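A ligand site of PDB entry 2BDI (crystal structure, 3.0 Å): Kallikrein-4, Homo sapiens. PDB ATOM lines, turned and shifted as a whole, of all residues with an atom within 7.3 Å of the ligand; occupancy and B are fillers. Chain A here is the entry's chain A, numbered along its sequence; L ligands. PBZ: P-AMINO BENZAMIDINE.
OD1 of Asn 174 lies close to SG of Cys 198, at 3.7 Å. The side-chain sulfur of Cys 173 forms a disulfide with the side-chain sulfur of Cys 198 (2.1 Å). The side-chain hydroxyl (OG) of Ser 172 lies within hydrogen-bond range of the side-chain hydroxyl (OH) of Tyr 207 (2.6 Å). The backbone NH of Ser 192 lies within hydrogen-bond range of the backbone carbonyl oxygen of Val 206 (3.2 Å). The side-chain amide oxygen of Asn 174 sits close to the side-chain sulfur of Cys 173, at 3.6 Å. The backbone carbonyl oxygen of Gly 205 is in hydrogen-bond range of the backbone NH of Ala 163 (3.1 Å). The side-chain carboxylate of Asp 86 sits at hydrogen-bond distance from a ring nitrogen (ND1) of His 41 (2.6 Å). The backbone NH (N) of Lys 195 sits at hydrogen-bond distance from the side-chain hydroxyl (OH) of Tyr 152.
N1 of the ligand lies within hydrogen-bond range of OG of Ser 177. N2 of the ligand sits at hydrogen-bond distance from SG of Cys 198, 2.7 Å away. O of Ser 172 sits at hydrogen-bond distance from N2 of the ligand (3.1 Å). N2 of the ligand is in salt-bridge range of OD2 of Asp 171 (3.1 Å). O of Ser 192 sits at hydrogen-bond distance from N1 of the ligand.
Residues that only touch the ligand: Phe 193 (3.1 Å), Asn 174 (3.5 Å), Cys 173 (3.5 Å), Gly 194 (3.6 Å), Gly 205 (3.8 Å), His 41 (3.9 Å) and Lys 195 (3.999 Å). The nearest printed residue that does not touch the ligand is Val 191 (4.02 Å).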
ATOM      1  N   ILE A   2     -24.608   2.721 -26.725  1.00  0.00           N
ATOM      2  CA  ILE A   2     -25.704   1.909 -27.240  1.00  0.00           C
ATOM      3  C   ILE A   2     -25.493   1.593 -28.711  1.00  0.00           C
ATOM      4  O   ILE A   2     -25.269   2.512 -29.514  1.00  0.00           O
ATOM      5  CB  ILE A   2     -27.047   2.652 -27.059  1.00  0.00           C
ATOM      6  CG1 ILE A   2     -27.316   2.939 -25.555  1.00  0.00           C
ATOM      7  CG2 ILE A   2     -28.179   1.772 -27.651  1.00  0.00           C
ATOM      8  CD1 ILE A   2     -27.444   1.709 -24.695  1.00  0.00           C
ATOM      9  N   HIS A  41     -20.775  17.077 -13.582  1.00  0.00           N
ATOM     10  CA  HIS A  41     -21.581  16.247 -12.760  1.00  0.00           C
ATOM     11  C   HIS A  41     -20.915  14.970 -12.367  1.00  0.00           C
ATOM     12  O   HIS A  41     -21.585  14.075 -11.974  1.00  0.00           O
ATOM     13  CB  HIS A  41     -22.907  15.988 -13.420  1.00  0.00           C
ATOM     14  CG  HIS A  41     -22.870  14.948 -14.473  1.00  0.00           C
ATOM     15  ND1 HIS A  41     -22.799  15.253 -15.821  1.00  0.00           N
ATOM     16  CD2 HIS A  41     -23.082  13.606 -14.397  1.00  0.00           C
ATOM     17  CE1 HIS A  41     -23.002  14.152 -16.520  1.00  0.00           C
ATOM     18  NE2 HIS A  41     -23.177  13.128 -15.671  1.00  0.00           N
ATOM     19  N   ASP A  86     -21.680  21.778 -18.153  1.00  0.00           N
ATOM     20  CA  ASP A  86     -21.322  20.554 -17.492  1.00  0.00           C
ATOM     21  C   ASP A  86     -19.884  20.114 -17.751  1.00  0.00           C
ATOM     22  O   ASP A  86     -19.674  19.021 -18.149  1.00  0.00           O
ATOM     23  CB  ASP A  86     -22.295  19.491 -17.946  1.00  0.00           C
ATOM     24  CG  ASP A  86     -22.172  18.212 -17.162  1.00  0.00           C
ATOM     25  OD1 ASP A  86     -21.338  18.175 -16.220  1.00  0.00           O
ATOM     26  OD2 ASP A  86     -22.944  17.214 -17.492  1.00  0.00           O
ATOM     27  N   TYR A 152     -34.990  20.255 -27.109  1.00  0.00           N
ATOM     28  CA  TYR A 152     -34.620  20.221 -25.699  1.00  0.00           C
ATOM     29  C   TYR A 152     -34.951  21.488 -24.969  1.00  0.00           C
ATOM     30  O   TYR A 152     -34.463  21.684 -23.857  1.00  0.00           O
ATOM     31  CB  TYR A 152     -33.128  19.955 -25.584  1.00  0.00           C
ATOM     32  CG  TYR A 152     -32.775  18.523 -25.565  1.00  0.00           C
ATOM     33  CD1 TYR A 152     -32.821  17.801 -24.379  1.00  0.00           C
ATOM     34  CD2 TYR A 152     -32.356  17.849 -26.729  1.00  0.00           C
ATOM     35  CE1 TYR A 152     -32.486  16.473 -24.340  1.00  0.00           C
ATOM     36  CE2 TYR A 152     -31.985  16.470 -26.677  1.00  0.00           C
ATOM     37  CZ  TYR A 152     -32.071  15.825 -25.477  1.00  0.00           C
ATOM     38  OH  TYR A 152     -31.725  14.533 -25.330  1.00  0.00           O
ATOM     39  N   ALA A 163     -26.005  15.162 -30.708  1.00  0.00           N
ATOM     40  CA  ALA A 163     -25.386  14.314 -31.686  1.00  0.00           C
ATOM     41  C   ALA A 163     -26.047  12.975 -31.620  1.00  0.00           C
ATOM     42  O   ALA A 163     -26.339  12.470 -30.558  1.00  0.00           O
ATOM     43  CB  ALA A 163     -23.919  14.142 -31.399  1.00  0.00           C
ATOM     44  N   ASP A 171     -26.055   5.657 -29.630  1.00  0.00           N
ATOM     45  CA  ASP A 171     -25.981   6.745 -28.682  1.00  0.00           C
ATOM     46  C   ASP A 171     -25.169   6.410 -27.427  1.00  0.00           C
ATOM     47  O   ASP A 171     -24.826   5.269 -27.258  1.00  0.00           O
ATOM     48  CB  ASP A 171     -27.390   7.088 -28.271  1.00  0.00           C
ATOM     49  CG  ASP A 171     -27.451   8.207 -27.267  1.00  0.00           C
ATOM     50  OD1 ASP A 171     -26.666   9.259 -27.452  1.00  0.00           O
ATOM     51  OD2 ASP A 171     -28.302   7.988 -26.336  1.00  0.00           O
ATOM     52  N   SER A 172     -24.871   7.396 -26.584  1.00  0.00           N
ATOM     53  CA  SER A 172     -24.212   7.123 -25.352  1.00  0.00           C
ATOM     54  C   SER A 172     -25.298   6.754 -24.403  1.00  0.00           C
ATOM     55  O   SER A 172     -26.457   6.697 -24.699  1.00  0.00           O
ATOM     56  CB  SER A 172     -23.567   8.316 -24.794  1.00  0.00           C
ATOM     57  OG  SER A 172     -23.459   9.226 -25.806  1.00  0.00           O
ATOM     58  N   CYS A 173     -24.940   6.666 -23.184  1.00  0.00           N
ATOM     59  CA  CYS A 173     -25.830   6.246 -22.163  1.00  0.00           C
ATOM     60  C   CYS A 173     -25.195   6.264 -20.664  1.00  0.00           C
ATOM     61  O   CYS A 173     -24.049   6.623 -20.366  1.00  0.00           O
ATOM     62  CB  CYS A 173     -26.358   4.866 -22.599  1.00  0.00           C
ATOM     63  SG  CYS A 173     -27.923   4.465 -21.736  1.00  0.00           S
ATOM     64  N   ASN A 174     -25.974   5.903 -19.696  1.00  0.00           N
ATOM     65  CA  ASN A 174     -25.480   5.970 -18.345  1.00  0.00           C
ATOM     66  C   ASN A 174     -24.136   5.283 -18.163  1.00  0.00           C
ATOM     67  O   ASN A 174     -23.958   4.096 -18.519  1.00  0.00           O
ATOM     68  CB  ASN A 174     -26.487   5.300 -17.424  1.00  0.00           C
ATOM     69  CG  ASN A 174     -27.847   5.963 -17.502  1.00  0.00           C
ATOM     70  OD1 ASN A 174     -28.411   6.139 -18.607  1.00  0.00           O
ATOM     71  ND2 ASN A 174     -28.393   6.327 -16.359  1.00  0.00           N
ATOM     72  N   GLY A 175     -23.184   6.016 -17.553  1.00  0.00           N
ATOM     73  CA  GLY A 175     -21.875   5.424 -17.319  1.00  0.00           C
ATOM     74  C   GLY A 175     -20.918   5.960 -18.324  1.00  0.00           C
ATOM     75  O   GLY A 175     -19.737   5.684 -18.237  1.00  0.00           O
ATOM     76  N   ASP A 176     -21.381   6.730 -19.273  1.00  0.00           N
ATOM     77  CA  ASP A 176     -20.480   7.284 -20.272  1.00  0.00           C
ATOM     78  C   ASP A 176     -20.268   8.747 -20.014  1.00  0.00           C
ATOM     79  O   ASP A 176     -19.555   9.390 -20.763  1.00  0.00           O
ATOM     80  CB  ASP A 176     -21.094   7.110 -21.631  1.00  0.00           C
ATOM     81  CG  ASP A 176     -21.247   5.632 -22.032  1.00  0.00           C
ATOM     82  OD1 ASP A 176     -20.417   4.802 -21.663  1.00  0.00           O
ATOM     83  OD2 ASP A 176     -22.192   5.285 -22.764  1.00  0.00           O
ATOM     84  N   SER A 177     -20.876   9.250 -18.934  1.00  0.00           N
ATOM     85  CA  SER A 177     -20.812  10.660 -18.655  1.00  0.00           C
ATOM     86  C   SER A 177     -19.381  11.074 -18.637  1.00  0.00           C
ATOM     87  O   SER A 177     -18.549  10.341 -18.108  1.00  0.00           O
ATOM     88  CB  SER A 177     -21.456  10.946 -17.314  1.00  0.00           C
ATOM     89  OG  SER A 177     -22.895  10.922 -17.315  1.00  0.00           O
ATOM     90  N   GLY A 178     -19.074  12.251 -19.216  1.00  0.00           N
ATOM     91  CA  GLY A 178     -17.696  12.766 -19.207  1.00  0.00           C
ATOM     92  C   GLY A 178     -16.851  12.141 -20.245  1.00  0.00           C
ATOM     93  O   GLY A 178     -15.738  12.541 -20.418  1.00  0.00           O
ATOM     94  N   VAL A 191     -19.711  13.544 -22.952  1.00  0.00           N
ATOM     95  CA  VAL A 191     -21.007  12.966 -22.706  1.00  0.00           C
ATOM     96  C   VAL A 191     -21.610  13.648 -21.481  1.00  0.00           C
ATOM     97  O   VAL A 191     -21.116  13.464 -20.434  1.00  0.00           O
ATOM     98  CB  VAL A 191     -20.807  11.536 -22.389  1.00  0.00           C
ATOM     99  CG1 VAL A 191     -22.100  10.885 -21.941  1.00  0.00           C
ATOM    100  CG2 VAL A 191     -20.224  10.923 -23.560  1.00  0.00           C
ATOM    101  N   SER A 192     -22.697  14.394 -21.640  1.00  0.00           N
ATOM    102  CA  SER A 192     -23.409  15.158 -20.553  1.00  0.00           C
ATOM    103  C   SER A 192     -24.715  14.542 -20.122  1.00  0.00           C
ATOM    104  O   SER A 192     -24.775  14.014 -19.047  1.00  0.00           O
ATOM    105  CB  SER A 192     -23.720  16.553 -21.004  1.00  0.00           C
ATOM    106  OG  SER A 192     -24.146  17.357 -19.912  1.00  0.00           O
ATOM    107  N   PHE A 193     -25.759  14.607 -20.930  1.00  0.00           N
ATOM    108  CA  PHE A 193     -27.018  13.977 -20.571  1.00  0.00           C
ATOM    109  C   PHE A 193     -27.846  13.709 -21.824  1.00  0.00           C
ATOM    110  O   PHE A 193     -27.465  14.040 -22.969  1.00  0.00           O
ATOM    111  CB  PHE A 193     -27.786  14.930 -19.666  1.00  0.00           C
ATOM    112  CG  PHE A 193     -28.317  16.133 -20.372  1.00  0.00           C
ATOM    113  CD1 PHE A 193     -29.571  16.123 -20.937  1.00  0.00           C
ATOM    114  CD2 PHE A 193     -27.584  17.296 -20.413  1.00  0.00           C
ATOM    115  CE1 PHE A 193     -30.054  17.300 -21.521  1.00  0.00           C
ATOM    116  CE2 PHE A 193     -28.127  18.495 -21.024  1.00  0.00           C
ATOM    117  CZ  PHE A 193     -29.321  18.497 -21.550  1.00  0.00           C
ATOM    118  N   GLY A 194     -29.034  13.177 -21.591  1.00  0.00           N
ATOM    119  CA  GLY A 194     -30.004  12.933 -22.659  1.00  0.00           C
ATOM    120  C   GLY A 194     -31.252  12.219 -22.109  1.00  0.00           C
ATOM    121  O   GLY A 194     -31.256  11.684 -20.986  1.00  0.00           O
ATOM    122  N   LYS A 195     -32.342  12.208 -22.875  1.00  0.00           N
ATOM    123  CA  LYS A 195     -33.579  11.522 -22.461  1.00  0.00           C
ATOM    124  C   LYS A 195     -33.383   9.999 -22.283  1.00  0.00           C
ATOM    125  O   LYS A 195     -32.425   9.384 -22.752  1.00  0.00           O
ATOM    126  N   ALA A 196     -34.258   9.405 -21.507  1.00  0.00           N
ATOM    127  CA  ALA A 196     -34.136   7.960 -21.221  1.00  0.00           C
ATOM    128  C   ALA A 196     -35.428   7.390 -21.596  1.00  0.00           C
ATOM    129  O   ALA A 196     -36.442   8.113 -21.553  1.00  0.00           O
ATOM    130  CB  ALA A 196     -33.934   7.690 -19.725  1.00  0.00           C
ATOM    131  N   PRO A 197     -35.420   6.140 -22.055  1.00  0.00           N
ATOM    132  CA  PRO A 197     -34.180   5.373 -22.176  1.00  0.00           C
ATOM    133  C   PRO A 197     -33.272   5.950 -23.275  1.00  0.00           C
ATOM    134  O   PRO A 197     -33.647   6.861 -24.056  1.00  0.00           O
ATOM    135  CB  PRO A 197     -34.698   3.984 -22.569  1.00  0.00           C
ATOM    136  CG  PRO A 197     -35.892   4.336 -23.438  1.00  0.00           C
ATOM    137  CD  PRO A 197     -36.583   5.395 -22.620  1.00  0.00           C
ATOM    138  N   CYS A 198     -32.070   5.397 -23.335  1.00  0.00           N
ATOM    139  CA  CYS A 198     -31.162   5.855 -24.353  1.00  0.00           C
ATOM    140  C   CYS A 198     -31.475   5.150 -25.646  1.00  0.00           C
ATOM    141  O   CYS A 198     -32.307   4.216 -25.647  1.00  0.00           O
ATOM    142  CB  CYS A 198     -29.776   5.589 -23.959  1.00  0.00           C
ATOM    143  SG  CYS A 198     -29.329   5.975 -22.238  1.00  0.00           S
ATOM    144  N   GLY A 199     -30.824   5.679 -26.716  1.00  0.00           N
ATOM    145  CA  GLY A 199     -31.000   5.184 -28.075  1.00  0.00           C
ATOM    146  C   GLY A 199     -32.356   5.311 -28.719  1.00  0.00           C
ATOM    147  O   GLY A 199     -32.740   4.478 -29.529  1.00  0.00           O
ATOM    148  N   GLN A 200     -33.105   6.346 -28.353  1.00  0.00           N
ATOM    149  CA  GLN A 200     -34.425   6.522 -28.948  1.00  0.00           C
ATOM    150  C   GLN A 200     -34.296   7.242 -30.246  1.00  0.00           C
ATOM    151  O   GLN A 200     -33.492   8.217 -30.415  1.00  0.00           O
ATOM    152  CB  GLN A 200     -35.304   7.332 -28.043  1.00  0.00           C
ATOM    153  CG  GLN A 200     -35.515   6.696 -26.749  1.00  0.00           C
ATOM    154  CD  GLN A 200     -36.481   7.586 -25.912  1.00  0.00           C
ATOM    155  OE1 GLN A 200     -36.335   7.689 -24.678  1.00  0.00           O
ATOM    156  NE2 GLN A 200     -37.439   8.211 -26.558  1.00  0.00           N
ATOM    157  N   VAL A 203     -34.237  11.220 -30.806  1.00  0.00           N
ATOM    158  CA  VAL A 203     -33.903  11.868 -29.559  1.00  0.00           C
ATOM    159  C   VAL A 203     -32.394  11.798 -29.388  1.00  0.00           C
ATOM    160  O   VAL A 203     -31.820  10.822 -28.803  1.00  0.00           O
ATOM    161  CB  VAL A 203     -34.530  11.124 -28.388  1.00  0.00           C
ATOM    162  CG1 VAL A 203     -34.577  12.025 -27.233  1.00  0.00           C
ATOM    163  CG2 VAL A 203     -35.832  10.643 -28.730  1.00  0.00           C
ATOM    164  N   PRO A 204     -31.734  12.811 -29.859  1.00  0.00           N
ATOM    165  CA  PRO A 204     -30.270  12.819 -29.761  1.00  0.00           C
ATOM    166  C   PRO A 204     -29.790  12.984 -28.334  1.00  0.00           C
ATOM    167  O   PRO A 204     -30.585  13.365 -27.465  1.00  0.00           O
ATOM    168  CB  PRO A 204     -29.844  14.005 -30.639  1.00  0.00           C
ATOM    169  CG  PRO A 204     -31.002  14.888 -30.565  1.00  0.00           C
ATOM    170  CD  PRO A 204     -32.261  13.977 -30.545  1.00  0.00           C
ATOM    171  N   GLY A 205     -28.491  12.719 -28.084  1.00  0.00           N
ATOM    172  CA  GLY A 205     -27.921  12.904 -26.768  1.00  0.00           C
ATOM    173  C   GLY A 205     -27.312  14.288 -26.714  1.00  0.00           C
ATOM    174  O   GLY A 205     -27.018  14.896 -27.786  1.00  0.00           O
ATOM    175  N   VAL A 206     -27.107  14.829 -25.471  1.00  0.00           N
ATOM    176  CA  VAL A 206     -26.513  16.160 -25.295  1.00  0.00           C
ATOM    177  C   VAL A 206     -25.050  15.983 -24.825  1.00  0.00           C
ATOM    178  O   VAL A 206     -24.719  15.066 -24.069  1.00  0.00           O
ATOM    179  CB  VAL A 206     -27.298  16.975 -24.328  1.00  0.00           C
ATOM    180  CG1 VAL A 206     -26.763  18.438 -24.360  1.00  0.00           C
ATOM    181  CG2 VAL A 206     -28.769  16.958 -24.713  1.00  0.00           C
ATOM    182  N   TYR A 207     -24.180  16.849 -25.347  1.00  0.00           N
ATOM    183  CA  TYR A 207     -22.745  16.804 -25.063  1.00  0.00           C
ATOM    184  C   TYR A 207     -22.284  18.241 -24.730  1.00  0.00           C
ATOM    185  O   TYR A 207     -22.823  19.220 -25.286  1.00  0.00           O
ATOM    186  CB  TYR A 207     -21.938  16.350 -26.296  1.00  0.00           C
ATOM    187  CG  TYR A 207     -22.223  14.961 -26.716  1.00  0.00           C
ATOM    188  CD1 TYR A 207     -23.295  14.687 -27.553  1.00  0.00           C
ATOM    189  CD2 TYR A 207     -21.458  13.881 -26.209  1.00  0.00           C
ATOM    190  CE1 TYR A 207     -23.630  13.373 -27.908  1.00  0.00           C
ATOM    191  CE2 TYR A 207     -21.797  12.546 -26.556  1.00  0.00           C
ATOM    192  CZ  TYR A 207     -22.888  12.308 -27.398  1.00  0.00           C
ATOM    193  OH  TYR A 207     -23.304  11.048 -27.646  1.00  0.00           O
HETATM  194  N2  PBZ L   1     -28.590   8.390 -23.299  1.00  0.00           N
HETATM  195  N3  PBZ L   1     -27.126  10.076 -24.283  1.00  0.00           N
HETATM  196  C7  PBZ L   1     -27.644   9.417 -23.137  1.00  0.00           C
HETATM  197  C4  PBZ L   1     -27.101   9.760 -21.634  1.00  0.00           C
HETATM  198  C2  PBZ L   1     -25.743  11.173 -20.266  1.00  0.00           C
HETATM  199  C3  PBZ L   1     -26.262  10.824 -21.474  1.00  0.00           C
HETATM  200  C5  PBZ L   1     -27.432   8.969 -20.389  1.00  0.00           C
HETATM  201  C6  PBZ L   1     -26.866   9.355 -19.110  1.00  0.00           C
HETATM  202  C1  PBZ L   1     -25.994  10.514 -19.140  1.00  0.00           C
HETATM  203  N1  PBZ L   1     -25.395  11.058 -18.103  1.00  0.00           N
